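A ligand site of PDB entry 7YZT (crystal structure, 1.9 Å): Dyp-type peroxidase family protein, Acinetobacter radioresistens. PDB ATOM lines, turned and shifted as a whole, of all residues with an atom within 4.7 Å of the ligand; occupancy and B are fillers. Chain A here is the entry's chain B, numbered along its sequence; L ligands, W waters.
The backbone NH of Ile 219 lies within hydrogen-bond range of the backbone carbonyl oxygen of Met 198, at 3.2 Å. The guanidinium group of Arg 236 lies within salt-bridge range of the side-chain carboxylate of Asp 144. The backbone NH (N) of Leu 250 is in hydrogen-bond range of a ring nitrogen (NE2) of His 181, 3.4 Å away. O of Leu 250 sits at hydrogen-bond distance from N of Tyr 179 (2.8 Å). OG1 of Thr 146 lies within hydrogen-bond range of OG of Ser 205, 2.7 Å away. The side-chain hydroxyl (OH) of Tyr 179 is in hydrogen-bond range of the side-chain amide oxygen (OE1) of Gln 177. O of Arg 236 sits at hydrogen-bond distance from ND2 of Asn 148 (2.8 Å). The backbone carbonyl oxygen of His 218 is in hydrogen-bond range of the side-chain hydroxyl of Thr 222 (3.2 Å).
Water W3 lies within hydrogen-bond range of the guanidinium group of Arg 236 (2.9 Å) and the side-chain carboxylate of Asp 144 (2.9 Å). Water W5 lies within hydrogen-bond range of an oxygen (O4) of the ligand (2.5 Å), the side-chain carboxylate (OE1) of Glu 231 (3.0 Å) and the side-chain carboxylate (OE1) of Glu 147 (3.1 Å). Water W4 bridges O4 of the ligand (2.6 Å) and O of Thr 222 (3.0 Å). Water W1 bridges an oxygen (O3) of the ligand and the guanidinium group (NH1) of Arg 200.
OD2 of Asp 138 touches C17 of the ligand (3.4 Å). CB of Phe 142 touches C9 of the ligand, 3.7 Å away. Ile 143 touches the ligand (O to C9, 3.3 Å). Asp 144 touches the ligand. Tyr 179 touches the ligand (OH to C24, 3.3 Å). His 181 touches the ligand. CD of Arg 200 touches C10 of the ligand (3.5 Å). CG2 of Ile 219 touches C1 of the ligand, at 3.8 Å. Thr 222 touches the ligand. Val 223 touches the ligand. CD2 of Leu 250 touches C15 of the ligand, 3.9 Å away. Phe 252 touches the ligand. Met 265 touches the ligand (CB to C26, 3.3 Å). Met 269 touches the ligand (SD to C21, 3.7 Å). CD2 of Leu 281 touches C14 of the ligand, at 3.7 Å. Val 285 touches the ligand. Hydrophobic or aromatic side chains that line the ligand: Phe 142, Tyr 179, His 181, His 218, Ile 219, Val 223, Leu 250, Phe 252, Met 265, Met 269, Leu 281 and Val 285. Within 4 Å of the ligand: Asp 138, Phe 142, Ile 143, Asp 144, Gly 145, Thr 146, Glu 147, Tyr 179, His 181, Arg 200, His 218, Ile 219, Thr 222, Val 223, Arg 236, Leu 250, Phe 252, Met 265, Met 269, Leu 281 and Val 285. Along chain A the residues within 4 Å of the ligand span positions 138 to 285. The nearest printed residue that does not touch the ligand is Met 198 (4.1 Å).
The backbone NH (N) of Gly 145 lies within hydrogen-bond range of an oxygen (O1) of the ligand (2.7 Å). O1 of the ligand is in salt-bridge range of NH1 of Arg 236, at 2.8 Å. An oxygen (O1) of the ligand sits close to the backbone NH of Thr 146, 3.3 Å away. A ring nitrogen (NE2) of His 218 is bound to an iron atom (FE1) of the ligand, 2.3 Å away. The backbone NH of Glu 147 sits at hydrogen-bond distance from an oxygen (O2) of the ligand, 2.9 Å away.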
ATOM      1  N   ASP A 138     -24.093 -16.402 -31.293  1.00  0.00           N
ATOM      2  CA  ASP A 138     -24.257 -16.486 -29.852  1.00  0.00           C
ATOM      3  C   ASP A 138     -25.321 -17.547 -29.540  1.00  0.00           C
ATOM      4  O   ASP A 138     -26.143 -17.898 -30.384  1.00  0.00           O
ATOM      5  CB  ASP A 138     -24.660 -15.102 -29.314  1.00  0.00           C
ATOM      6  CG  ASP A 138     -24.973 -15.099 -27.822  1.00  0.00           C
ATOM      7  OD1 ASP A 138     -24.032 -15.002 -27.011  1.00  0.00           O
ATOM      8  OD2 ASP A 138     -26.165 -15.116 -27.460  1.00  0.00           O
ATOM      9  N   PHE A 142     -28.579 -15.702 -32.296  1.00  0.00           N
ATOM     10  CA  PHE A 142     -28.306 -14.547 -33.145  1.00  0.00           C
ATOM     11  C   PHE A 142     -26.834 -14.530 -33.545  1.00  0.00           C
ATOM     12  O   PHE A 142     -25.965 -14.877 -32.752  1.00  0.00           O
ATOM     13  CB  PHE A 142     -28.654 -13.244 -32.413  1.00  0.00           C
ATOM     14  CG  PHE A 142     -30.117 -12.927 -32.446  1.00  0.00           C
ATOM     15  CD1 PHE A 142     -31.000 -13.631 -31.633  1.00  0.00           C
ATOM     16  CD2 PHE A 142     -30.622 -11.949 -33.289  1.00  0.00           C
ATOM     17  CE1 PHE A 142     -32.362 -13.373 -31.664  1.00  0.00           C
ATOM     18  CE2 PHE A 142     -31.973 -11.674 -33.321  1.00  0.00           C
ATOM     19  CZ  PHE A 142     -32.854 -12.379 -32.499  1.00  0.00           C
ATOM     20  N   ILE A 143     -26.587 -14.127 -34.788  1.00  0.00           N
ATOM     21  CA  ILE A 143     -25.211 -14.013 -35.261  1.00  0.00           C
ATOM     22  C   ILE A 143     -24.501 -12.887 -34.515  1.00  0.00           C
ATOM     23  O   ILE A 143     -25.043 -11.775 -34.374  1.00  0.00           O
ATOM     24  CB  ILE A 143     -25.177 -13.765 -36.775  1.00  0.00           C
ATOM     25  CG1 ILE A 143     -25.742 -14.963 -37.545  1.00  0.00           C
ATOM     26  CG2 ILE A 143     -23.745 -13.440 -37.235  1.00  0.00           C
ATOM     27  CD1 ILE A 143     -26.001 -14.661 -39.010  1.00  0.00           C
ATOM     28  N   ASP A 144     -23.300 -13.160 -34.042  1.00  0.00           N
ATOM     29  CA  ASP A 144     -22.472 -12.163 -33.363  1.00  0.00           C
ATOM     30  C   ASP A 144     -21.346 -11.776 -34.299  1.00  0.00           C
ATOM     31  O   ASP A 144     -20.609 -12.645 -34.767  1.00  0.00           O
ATOM     32  CB  ASP A 144     -21.908 -12.716 -32.054  1.00  0.00           C
ATOM     33  CG  ASP A 144     -21.252 -11.647 -31.204  1.00  0.00           C
ATOM     34  OD1 ASP A 144     -21.728 -10.487 -31.215  1.00  0.00           O
ATOM     35  OD2 ASP A 144     -20.262 -11.964 -30.520  1.00  0.00           O
ATOM     36  N   GLY A 145     -21.217 -10.479 -34.561  1.00  0.00           N
ATOM     37  CA  GLY A 145     -20.065  -9.959 -35.296  1.00  0.00           C
ATOM     38  C   GLY A 145     -20.393  -9.217 -36.570  1.00  0.00           C
ATOM     39  O   GLY A 145     -19.457  -8.733 -37.240  1.00  0.00           O
ATOM     40  N   THR A 146     -21.663  -9.095 -36.937  1.00  0.00           N
ATOM     41  CA  THR A 146     -22.051  -8.527 -38.226  1.00  0.00           C
ATOM     42  C   THR A 146     -21.429  -7.153 -38.478  1.00  0.00           C
ATOM     43  O   THR A 146     -20.932  -6.886 -39.577  1.00  0.00           O
ATOM     44  CB  THR A 146     -23.578  -8.454 -38.336  1.00  0.00           C
ATOM     45  OG1 THR A 146     -24.131  -9.768 -38.183  1.00  0.00           O
ATOM     46  CG2 THR A 146     -23.997  -7.870 -39.666  1.00  0.00           C
ATOM     47  N   GLU A 147     -21.450  -6.267 -37.487  1.00  0.00           N
ATOM     48  CA  GLU A 147     -20.940  -4.906 -37.662  1.00  0.00           C
ATOM     49  C   GLU A 147     -19.519  -4.727 -37.122  1.00  0.00           C
ATOM     50  O   GLU A 147     -18.992  -3.597 -37.101  1.00  0.00           O
ATOM     51  CB  GLU A 147     -21.901  -3.913 -37.019  1.00  0.00           C
ATOM     52  CG  GLU A 147     -23.062  -3.555 -37.940  1.00  0.00           C
ATOM     53  CD  GLU A 147     -22.600  -2.767 -39.155  1.00  0.00           C
ATOM     54  OE1 GLU A 147     -21.679  -1.915 -39.005  1.00  0.00           O
ATOM     55  OE2 GLU A 147     -23.122  -3.013 -40.262  1.00  0.00           O
ATOM     56  N   ASN A 148     -18.887  -5.807 -36.694  1.00  0.00           N
ATOM     57  CA  ASN A 148     -17.482  -5.776 -36.339  1.00  0.00           C
ATOM     58  C   ASN A 148     -16.633  -5.394 -37.557  1.00  0.00           C
ATOM     59  O   ASN A 148     -16.901  -5.877 -38.663  1.00  0.00           O
ATOM     60  CB  ASN A 148     -17.073  -7.165 -35.862  1.00  0.00           C
ATOM     61  CG  ASN A 148     -16.056  -7.156 -34.769  1.00  0.00           C
ATOM     62  OD1 ASN A 148     -15.883  -6.163 -34.059  1.00  0.00           O
ATOM     63  ND2 ASN A 148     -15.393  -8.289 -34.613  1.00  0.00           N
ATOM     64  N   PHE A 175     -10.953  -5.046 -23.005  1.00  0.00           N
ATOM     65  CA  PHE A 175     -12.072  -5.183 -22.078  1.00  0.00           C
ATOM     66  C   PHE A 175     -12.577  -6.617 -22.180  1.00  0.00           C
ATOM     67  O   PHE A 175     -12.967  -7.052 -23.261  1.00  0.00           O
ATOM     68  CB  PHE A 175     -13.182  -4.195 -22.427  1.00  0.00           C
ATOM     69  CG  PHE A 175     -14.492  -4.476 -21.735  1.00  0.00           C
ATOM     70  CD1 PHE A 175     -14.547  -4.648 -20.352  1.00  0.00           C
ATOM     71  CD2 PHE A 175     -15.675  -4.558 -22.466  1.00  0.00           C
ATOM     72  CE1 PHE A 175     -15.766  -4.914 -19.697  1.00  0.00           C
ATOM     73  CE2 PHE A 175     -16.889  -4.827 -21.824  1.00  0.00           C
ATOM     74  CZ  PHE A 175     -16.936  -4.992 -20.432  1.00  0.00           C
ATOM     75  N   GLN A 177     -15.125  -9.606 -20.270  1.00  0.00           N
ATOM     76  CA  GLN A 177     -16.256  -9.760 -19.352  1.00  0.00           C
ATOM     77  C   GLN A 177     -17.069 -10.974 -19.769  1.00  0.00           C
ATOM     78  O   GLN A 177     -17.587 -11.015 -20.890  1.00  0.00           O
ATOM     79  CB  GLN A 177     -17.122  -8.527 -19.364  1.00  0.00           C
ATOM     80  CG  GLN A 177     -18.311  -8.591 -18.447  1.00  0.00           C
ATOM     81  CD  GLN A 177     -18.857  -7.217 -18.182  1.00  0.00           C
ATOM     82  OE1 GLN A 177     -19.553  -6.649 -19.021  1.00  0.00           O
ATOM     83  NE2 GLN A 177     -18.485  -6.642 -17.044  1.00  0.00           N
ATOM     84  N   TYR A 179     -20.326 -13.307 -19.764  1.00  0.00           N
ATOM     85  CA  TYR A 179     -21.763 -13.226 -19.573  1.00  0.00           C
ATOM     86  C   TYR A 179     -22.358 -14.620 -19.438  1.00  0.00           C
ATOM     87  O   TYR A 179     -21.904 -15.556 -20.110  1.00  0.00           O
ATOM     88  CB  TYR A 179     -22.432 -12.492 -20.737  1.00  0.00           C
ATOM     89  CG  TYR A 179     -22.324 -10.991 -20.592  1.00  0.00           C
ATOM     90  CD1 TYR A 179     -21.130 -10.336 -20.844  1.00  0.00           C
ATOM     91  CD2 TYR A 179     -23.413 -10.234 -20.164  1.00  0.00           C
ATOM     92  CE1 TYR A 179     -21.014  -8.954 -20.687  1.00  0.00           C
ATOM     93  CE2 TYR A 179     -23.318  -8.851 -20.000  1.00  0.00           C
ATOM     94  CZ  TYR A 179     -22.113  -8.227 -20.271  1.00  0.00           C
ATOM     95  OH  TYR A 179     -21.985  -6.851 -20.107  1.00  0.00           O
ATOM     96  N   HIS A 181     -26.106 -16.527 -19.776  1.00  0.00           N
ATOM     97  CA  HIS A 181     -27.435 -16.323 -20.345  1.00  0.00           C
ATOM     98  C   HIS A 181     -28.491 -17.115 -19.584  1.00  0.00           C
ATOM     99  O   HIS A 181     -28.227 -18.199 -19.059  1.00  0.00           O
ATOM    100  CB  HIS A 181     -27.484 -16.717 -21.827  1.00  0.00           C
ATOM    101  CG  HIS A 181     -26.499 -15.993 -22.691  1.00  0.00           C
ATOM    102  ND1 HIS A 181     -26.667 -15.842 -24.048  1.00  0.00           N
ATOM    103  CD2 HIS A 181     -25.384 -15.303 -22.372  1.00  0.00           C
ATOM    104  CE1 HIS A 181     -25.660 -15.149 -24.542  1.00  0.00           C
ATOM    105  NE2 HIS A 181     -24.870 -14.807 -23.551  1.00  0.00           N
ATOM    106  N   MET A 198     -32.765  -7.393 -29.926  1.00  0.00           N
ATOM    107  CA  MET A 198     -31.412  -7.348 -30.443  1.00  0.00           C
ATOM    108  C   MET A 198     -31.239  -6.176 -31.415  1.00  0.00           C
ATOM    109  O   MET A 198     -30.197  -5.515 -31.416  1.00  0.00           O
ATOM    110  CB  MET A 198     -31.079  -8.666 -31.161  1.00  0.00           C
ATOM    111  CG  MET A 198     -30.838  -9.810 -30.213  1.00  0.00           C
ATOM    112  SD  MET A 198     -29.423  -9.594 -29.167  1.00  0.00           S
ATOM    113  CE  MET A 198     -29.352 -11.226 -28.412  1.00  0.00           C
ATOM    114  N   ARG A 200     -31.606  -6.739 -34.823  1.00  0.00           N
ATOM    115  CA  ARG A 200     -31.326  -7.406 -36.100  1.00  0.00           C
ATOM    116  C   ARG A 200     -32.218  -8.641 -36.198  1.00  0.00           C
ATOM    117  O   ARG A 200     -32.735  -9.143 -35.200  1.00  0.00           O
ATOM    118  CB  ARG A 200     -29.838  -7.801 -36.225  1.00  0.00           C
ATOM    119  CG  ARG A 200     -28.821  -6.685 -35.888  1.00  0.00           C
ATOM    120  CD  ARG A 200     -27.362  -6.961 -36.315  1.00  0.00           C
ATOM    121  NE  ARG A 200     -27.202  -6.933 -37.774  1.00  0.00           N
ATOM    122  CZ  ARG A 200     -26.828  -5.863 -38.466  1.00  0.00           C
ATOM    123  NH1 ARG A 200     -26.529  -4.717 -37.881  1.00  0.00           N
ATOM    124  NH2 ARG A 200     -26.820  -5.927 -39.803  1.00  0.00           N
ATOM    125  N   SER A 205     -29.426 -11.804 -39.565  1.00  0.00           N
ATOM    126  CA  SER A 205     -28.757 -10.628 -38.990  1.00  0.00           C
ATOM    127  C   SER A 205     -28.928  -9.395 -39.895  1.00  0.00           C
ATOM    128  O   SER A 205     -28.013  -8.576 -40.045  1.00  0.00           O
ATOM    129  CB  SER A 205     -27.277 -10.885 -38.700  1.00  0.00           C
ATOM    130  OG  SER A 205     -26.814  -9.942 -37.720  1.00  0.00           O
ATOM    131  N   HIS A 218     -30.479  -3.855 -28.290  1.00  0.00           N
ATOM    132  CA  HIS A 218     -29.070  -3.977 -27.947  1.00  0.00           C
ATOM    133  C   HIS A 218     -28.208  -3.104 -28.846  1.00  0.00           C
ATOM    134  O   HIS A 218     -27.380  -2.310 -28.356  1.00  0.00           O
ATOM    135  CB  HIS A 218     -28.645  -5.434 -28.026  1.00  0.00           C
ATOM    136  CG  HIS A 218     -27.216  -5.648 -27.681  1.00  0.00           C
ATOM    137  ND1 HIS A 218     -26.706  -5.377 -26.430  1.00  0.00           N
ATOM    138  CD2 HIS A 218     -26.185  -6.121 -28.422  1.00  0.00           C
ATOM    139  CE1 HIS A 218     -25.421  -5.673 -26.411  1.00  0.00           C
ATOM    140  NE2 HIS A 218     -25.084  -6.115 -27.601  1.00  0.00           N
ATOM    141  N   ILE A 219     -28.374  -3.205 -30.164  1.00  0.00           N
ATOM    142  CA  ILE A 219     -27.498  -2.443 -31.051  1.00  0.00           C
ATOM    143  C   ILE A 219     -27.896  -0.975 -31.161  1.00  0.00           C
ATOM    144  O   ILE A 219     -27.122  -0.173 -31.691  1.00  0.00           O
ATOM    145  CB  ILE A 219     -27.410  -3.051 -32.460  1.00  0.00           C
ATOM    146  CG1 ILE A 219     -28.716  -2.869 -33.241  1.00  0.00           C
ATOM    147  CG2 ILE A 219     -26.963  -4.526 -32.399  1.00  0.00           C
ATOM    148  CD1 ILE A 219     -28.527  -2.999 -34.763  1.00  0.00           C
ATOM    149  N   THR A 222     -25.464   0.000 -28.237  1.00  0.00           N
ATOM    150  CA  THR A 222     -24.037  -0.168 -28.448  1.00  0.00           C
ATOM    151  C   THR A 222     -23.504   0.580 -29.671  1.00  0.00           C
ATOM    152  O   THR A 222     -22.296   0.546 -29.919  1.00  0.00           O
ATOM    153  CB  THR A 222     -23.685  -1.655 -28.570  1.00  0.00           C
ATOM    154  OG1 THR A 222     -24.475  -2.275 -29.611  1.00  0.00           O
ATOM    155  CG2 THR A 222     -23.957  -2.363 -27.246  1.00  0.00           C
ATOM    156  N   VAL A 223     -24.368   1.235 -30.444  1.00  0.00           N
ATOM    157  CA  VAL A 223     -23.935   2.152 -31.495  1.00  0.00           C
ATOM    158  C   VAL A 223     -23.808   3.537 -30.863  1.00  0.00           C
ATOM    159  O   VAL A 223     -24.794   4.077 -30.350  1.00  0.00           O
ATOM    160  CB  VAL A 223     -24.921   2.168 -32.668  1.00  0.00           C
ATOM    161  CG1 VAL A 223     -24.707   3.378 -33.564  1.00  0.00           C
ATOM    162  CG2 VAL A 223     -24.814   0.872 -33.490  1.00  0.00           C
ATOM    163  N   GLU A 231     -19.461   7.779 -35.906  1.00  0.00           N
ATOM    164  CA  GLU A 231     -19.573   6.539 -35.143  1.00  0.00           C
ATOM    165  C   GLU A 231     -18.227   6.141 -34.554  1.00  0.00           C
ATOM    166  O   GLU A 231     -17.183   6.324 -35.185  1.00  0.00           O
ATOM    167  CB  GLU A 231     -20.115   5.405 -36.008  1.00  0.00           C
ATOM    168  CG  GLU A 231     -21.515   4.957 -35.564  1.00  0.00           C
ATOM    169  CD  GLU A 231     -22.050   3.742 -36.326  1.00  0.00           C
ATOM    170  OE1 GLU A 231     -21.316   2.729 -36.441  1.00  0.00           O
ATOM    171  OE2 GLU A 231     -23.200   3.824 -36.822  1.00  0.00           O
ATOM    172  N   ILE A 234     -15.323  -0.471 -31.836  1.00  0.00           N
ATOM    173  CA  ILE A 234     -14.403  -1.358 -31.135  1.00  0.00           C
ATOM    174  C   ILE A 234     -14.223  -2.627 -31.966  1.00  0.00           C
ATOM    175  O   ILE A 234     -14.985  -2.902 -32.893  1.00  0.00           O
ATOM    176  CB  ILE A 234     -14.880  -1.702 -29.692  1.00  0.00           C
ATOM    177  CG1 ILE A 234     -16.204  -2.479 -29.733  1.00  0.00           C
ATOM    178  CG2 ILE A 234     -15.027  -0.415 -28.837  1.00  0.00           C
ATOM    179  CD1 ILE A 234     -16.699  -2.885 -28.368  1.00  0.00           C
ATOM    180  N   ARG A 236     -14.314  -6.444 -31.584  1.00  0.00           N
ATOM    181  CA  ARG A 236     -14.745  -7.518 -30.695  1.00  0.00           C
ATOM    182  C   ARG A 236     -14.130  -8.856 -31.114  1.00  0.00           C
ATOM    183  O   ARG A 236     -13.973  -9.148 -32.299  1.00  0.00           O
ATOM    184  CB  ARG A 236     -16.267  -7.650 -30.676  1.00  0.00           C
ATOM    185  CG  ARG A 236     -16.955  -6.421 -30.035  1.00  0.00           C
ATOM    186  CD  ARG A 236     -18.468  -6.462 -30.187  1.00  0.00           C
ATOM    187  NE  ARG A 236     -18.862  -6.077 -31.532  1.00  0.00           N
ATOM    188  CZ  ARG A 236     -19.788  -6.709 -32.255  1.00  0.00           C
ATOM    189  NH1 ARG A 236     -20.440  -7.755 -31.767  1.00  0.00           N
ATOM    190  NH2 ARG A 236     -20.061  -6.261 -33.482  1.00  0.00           N
ATOM    191  N   LEU A 250     -21.701 -16.009 -23.305  1.00  0.00           N
ATOM    192  CA  LEU A 250     -20.763 -15.398 -24.213  1.00  0.00           C
ATOM    193  C   LEU A 250     -19.605 -14.860 -23.388  1.00  0.00           C
ATOM    194  O   LEU A 250     -19.830 -14.190 -22.372  1.00  0.00           O
ATOM    195  CB  LEU A 250     -21.400 -14.251 -25.021  1.00  0.00           C
ATOM    196  CG  LEU A 250     -20.511 -13.561 -26.072  1.00  0.00           C
ATOM    197  CD1 LEU A 250     -20.303 -14.483 -27.277  1.00  0.00           C
ATOM    198  CD2 LEU A 250     -21.125 -12.239 -26.534  1.00  0.00           C
ATOM    199  N   PHE A 252     -17.376 -12.083 -23.538  1.00  0.00           N
ATOM    200  CA  PHE A 252     -17.220 -10.857 -24.296  1.00  0.00           C
ATOM    201  C   PHE A 252     -15.801 -10.337 -24.163  1.00  0.00           C
ATOM    202  O   PHE A 252     -15.264 -10.249 -23.063  1.00  0.00           O
ATOM    203  CB  PHE A 252     -18.200  -9.769 -23.836  1.00  0.00           C
ATOM    204  CG  PHE A 252     -18.122  -8.549 -24.686  1.00  0.00           C
ATOM    205  CD1 PHE A 252     -18.883  -8.441 -25.834  1.00  0.00           C
ATOM    206  CD2 PHE A 252     -17.241  -7.517 -24.380  1.00  0.00           C
ATOM    207  CE1 PHE A 252     -18.782  -7.335 -26.644  1.00  0.00           C
ATOM    208  CE2 PHE A 252     -17.130  -6.406 -25.203  1.00  0.00           C
ATOM    209  CZ  PHE A 252     -17.909  -6.310 -26.316  1.00  0.00           C
ATOM    210  N   MET A 265     -20.480   2.819 -24.131  1.00  0.00           N
ATOM    211  CA  MET A 265     -21.395   1.727 -24.434  1.00  0.00           C
ATOM    212  C   MET A 265     -21.925   1.060 -23.168  1.00  0.00           C
ATOM    213  O   MET A 265     -23.122   0.768 -23.086  1.00  0.00           O
ATOM    214  CB  MET A 265     -20.754   0.674 -25.352  1.00  0.00           C
ATOM    215  CG  MET A 265     -19.942   1.207 -26.516  1.00  0.00           C
ATOM    216  SD  MET A 265     -19.070  -0.105 -27.430  1.00  0.00           S
ATOM    217  CE  MET A 265     -18.981   0.637 -29.072  1.00  0.00           C
ATOM    218  N   LEU A 266     -21.053   0.813 -22.181  1.00  0.00           N
ATOM    219  CA  LEU A 266     -21.501   0.213 -20.932  1.00  0.00           C
ATOM    220  C   LEU A 266     -22.476   1.115 -20.192  1.00  0.00           C
ATOM    221  O   LEU A 266     -23.489   0.634 -19.656  1.00  0.00           O
ATOM    222  CB  LEU A 266     -20.297  -0.113 -20.043  1.00  0.00           C
ATOM    223  CG  LEU A 266     -19.357  -1.204 -20.565  1.00  0.00           C
ATOM    224  CD1 LEU A 266     -18.139  -1.319 -19.672  1.00  0.00           C
ATOM    225  CD2 LEU A 266     -20.116  -2.539 -20.677  1.00  0.00           C
ATOM    226  N   MET A 269     -25.756   0.684 -22.032  1.00  0.00           N
ATOM    227  CA  MET A 269     -26.396  -0.612 -21.816  1.00  0.00           C
ATOM    228  C   MET A 269     -27.001  -0.700 -20.424  1.00  0.00           C
ATOM    229  O   MET A 269     -28.164  -1.101 -20.283  1.00  0.00           O
ATOM    230  CB  MET A 269     -25.432  -1.784 -22.040  1.00  0.00           C
ATOM    231  CG  MET A 269     -24.909  -1.951 -23.474  1.00  0.00           C
ATOM    232  SD  MET A 269     -23.659  -3.259 -23.587  1.00  0.00           S
ATOM    233  CE  MET A 269     -24.486  -4.616 -22.746  1.00  0.00           C
ATOM    234  N   LEU A 281     -31.630  -6.300 -23.648  1.00  0.00           N
ATOM    235  CA  LEU A 281     -30.972  -7.609 -23.611  1.00  0.00           C
ATOM    236  C   LEU A 281     -30.483  -7.953 -22.217  1.00  0.00           C
ATOM    237  O   LEU A 281     -30.350  -9.144 -21.887  1.00  0.00           O
ATOM    238  CB  LEU A 281     -29.810  -7.660 -24.611  1.00  0.00           C
ATOM    239  CG  LEU A 281     -28.987  -8.964 -24.690  1.00  0.00           C
ATOM    240  CD1 LEU A 281     -29.838 -10.132 -25.088  1.00  0.00           C
ATOM    241  CD2 LEU A 281     -27.792  -8.813 -25.629  1.00  0.00           C
ATOM    242  N   VAL A 285     -29.275 -11.698 -19.838  1.00  0.00           N
ATOM    243  CA  VAL A 285     -27.864 -12.071 -19.701  1.00  0.00           C
ATOM    244  C   VAL A 285     -27.306 -11.300 -18.511  1.00  0.00           C
ATOM    245  O   VAL A 285     -27.769 -10.203 -18.185  1.00  0.00           O
ATOM    246  CB  VAL A 285     -27.040 -11.793 -20.979  1.00  0.00           C
ATOM    247  CG1 VAL A 285     -27.616 -12.519 -22.189  1.00  0.00           C
ATOM    248  CG2 VAL A 285     -26.947 -10.267 -21.240  1.00  0.00           C
HETATM  249  C1  LIG L   1     -23.646  -6.123 -31.610  1.00  0.00           C
HETATM  250  C2  LIG L   1     -24.906  -9.963 -28.901  1.00  0.00           C
HETATM  251  C3  LIG L   1     -22.762  -7.871 -25.037  1.00  0.00           C
HETATM  252  C4  LIG L   1     -21.040  -4.359 -27.889  1.00  0.00           C
HETATM  253  C5  LIG L   1     -24.223  -7.309 -31.219  1.00  0.00           C
HETATM  254  C6  LIG L   1     -25.086  -8.153 -32.024  1.00  0.00           C
HETATM  255  C7  LIG L   1     -25.443  -9.208 -31.283  1.00  0.00           C
HETATM  256  C8  LIG L   1     -24.804  -9.089 -29.978  1.00  0.00           C
HETATM  257  C9  LIG L   1     -26.365 -10.383 -31.723  1.00  0.00           C
HETATM  258  C10 LIG L   1     -25.499  -7.867 -33.483  1.00  0.00           C
HETATM  259  C11 LIG L   1     -24.489  -8.464 -34.457  1.00  0.00           C
HETATM  260  C12 LIG L   1     -23.210  -7.654 -34.514  1.00  0.00           C
HETATM  261  O1  LIG L   1     -22.213  -8.092 -33.880  1.00  0.00           O
HETATM  262  O2  LIG L   1     -23.183  -6.580 -35.187  1.00  0.00           O
HETATM  263  C13 LIG L   1     -24.442  -9.710 -27.616  1.00  0.00           C
HETATM  264  C14 LIG L   1     -24.646 -10.580 -26.463  1.00  0.00           C
HETATM  265  C15 LIG L   1     -24.055  -9.995 -25.406  1.00  0.00           C
HETATM  266  C16 LIG L   1     -23.447  -8.748 -25.841  1.00  0.00           C
HETATM  267  C17 LIG L   1     -25.430 -11.909 -26.524  1.00  0.00           C
HETATM  268  C18 LIG L   1     -23.944 -10.466 -23.939  1.00  0.00           C
HETATM  269  C19 LIG L   1     -24.243 -11.695 -23.527  1.00  0.00           C
HETATM  270  C20 LIG L   1     -22.081  -6.745 -25.449  1.00  0.00           C
HETATM  271  C21 LIG L   1     -21.237  -5.889 -24.647  1.00  0.00           C
HETATM  272  C22 LIG L   1     -20.793  -4.910 -25.428  1.00  0.00           C
HETATM  273  C23 LIG L   1     -21.293  -5.122 -26.770  1.00  0.00           C
HETATM  274  C24 LIG L   1     -20.915  -6.030 -23.138  1.00  0.00           C
HETATM  275  C25 LIG L   1     -19.826  -3.816 -24.940  1.00  0.00           C
HETATM  276  C26 LIG L   1     -20.143  -2.529 -24.984  1.00  0.00           C
HETATM  277  C27 LIG L   1     -21.570  -4.550 -29.155  1.00  0.00           C
HETATM  278  C28 LIG L   1     -21.260  -3.753 -30.331  1.00  0.00           C
HETATM  279  C29 LIG L   1     -21.972  -4.233 -31.356  1.00  0.00           C
HETATM  280  C30 LIG L   1     -22.766  -5.348 -30.874  1.00  0.00           C
HETATM  281  C31 LIG L   1     -20.258  -2.575 -30.363  1.00  0.00           C
HETATM  282  C32 LIG L   1     -21.974  -3.673 -32.804  1.00  0.00           C
HETATM  283  C33 LIG L   1     -23.205  -2.769 -32.967  1.00  0.00           C
HETATM  284  C34 LIG L   1     -23.126  -1.960 -34.246  1.00  0.00           C
HETATM  285  O3  LIG L   1     -24.043  -2.108 -35.105  1.00  0.00           O
HETATM  286  O4  LIG L   1     -22.150  -1.166 -34.419  1.00  0.00           O
HETATM  287  N1  LIG L   1     -24.082  -7.911 -29.971  1.00  0.00           N
HETATM  288  N2  LIG L   1     -23.703  -8.616 -27.203  1.00  0.00           N
HETATM  289  N3  LIG L   1     -22.091  -6.243 -26.743  1.00  0.00           N
HETATM  290  N4  LIG L   1     -22.486  -5.495 -29.522  1.00  0.00           N
HETATM  291 FE1  LIG L   1     -23.127  -7.025 -28.364  1.00  0.00          FE
HETATM  292  O   HOH W   1     -25.097  -4.558 -35.321  1.00  0.00           O
HETATM  293  O   HOH W   2     -24.811  -0.433 -36.879  1.00  0.00           O
HETATM  294  O   HOH W   3     -21.292  -8.521 -29.064  1.00  0.00           O
HETATM  295  O   HOH W   4     -20.838  -0.011 -32.539  1.00  0.00           O
HETATM  296  O   HOH W   5     -21.098  -0.268 -36.490  1.00  0.00           O
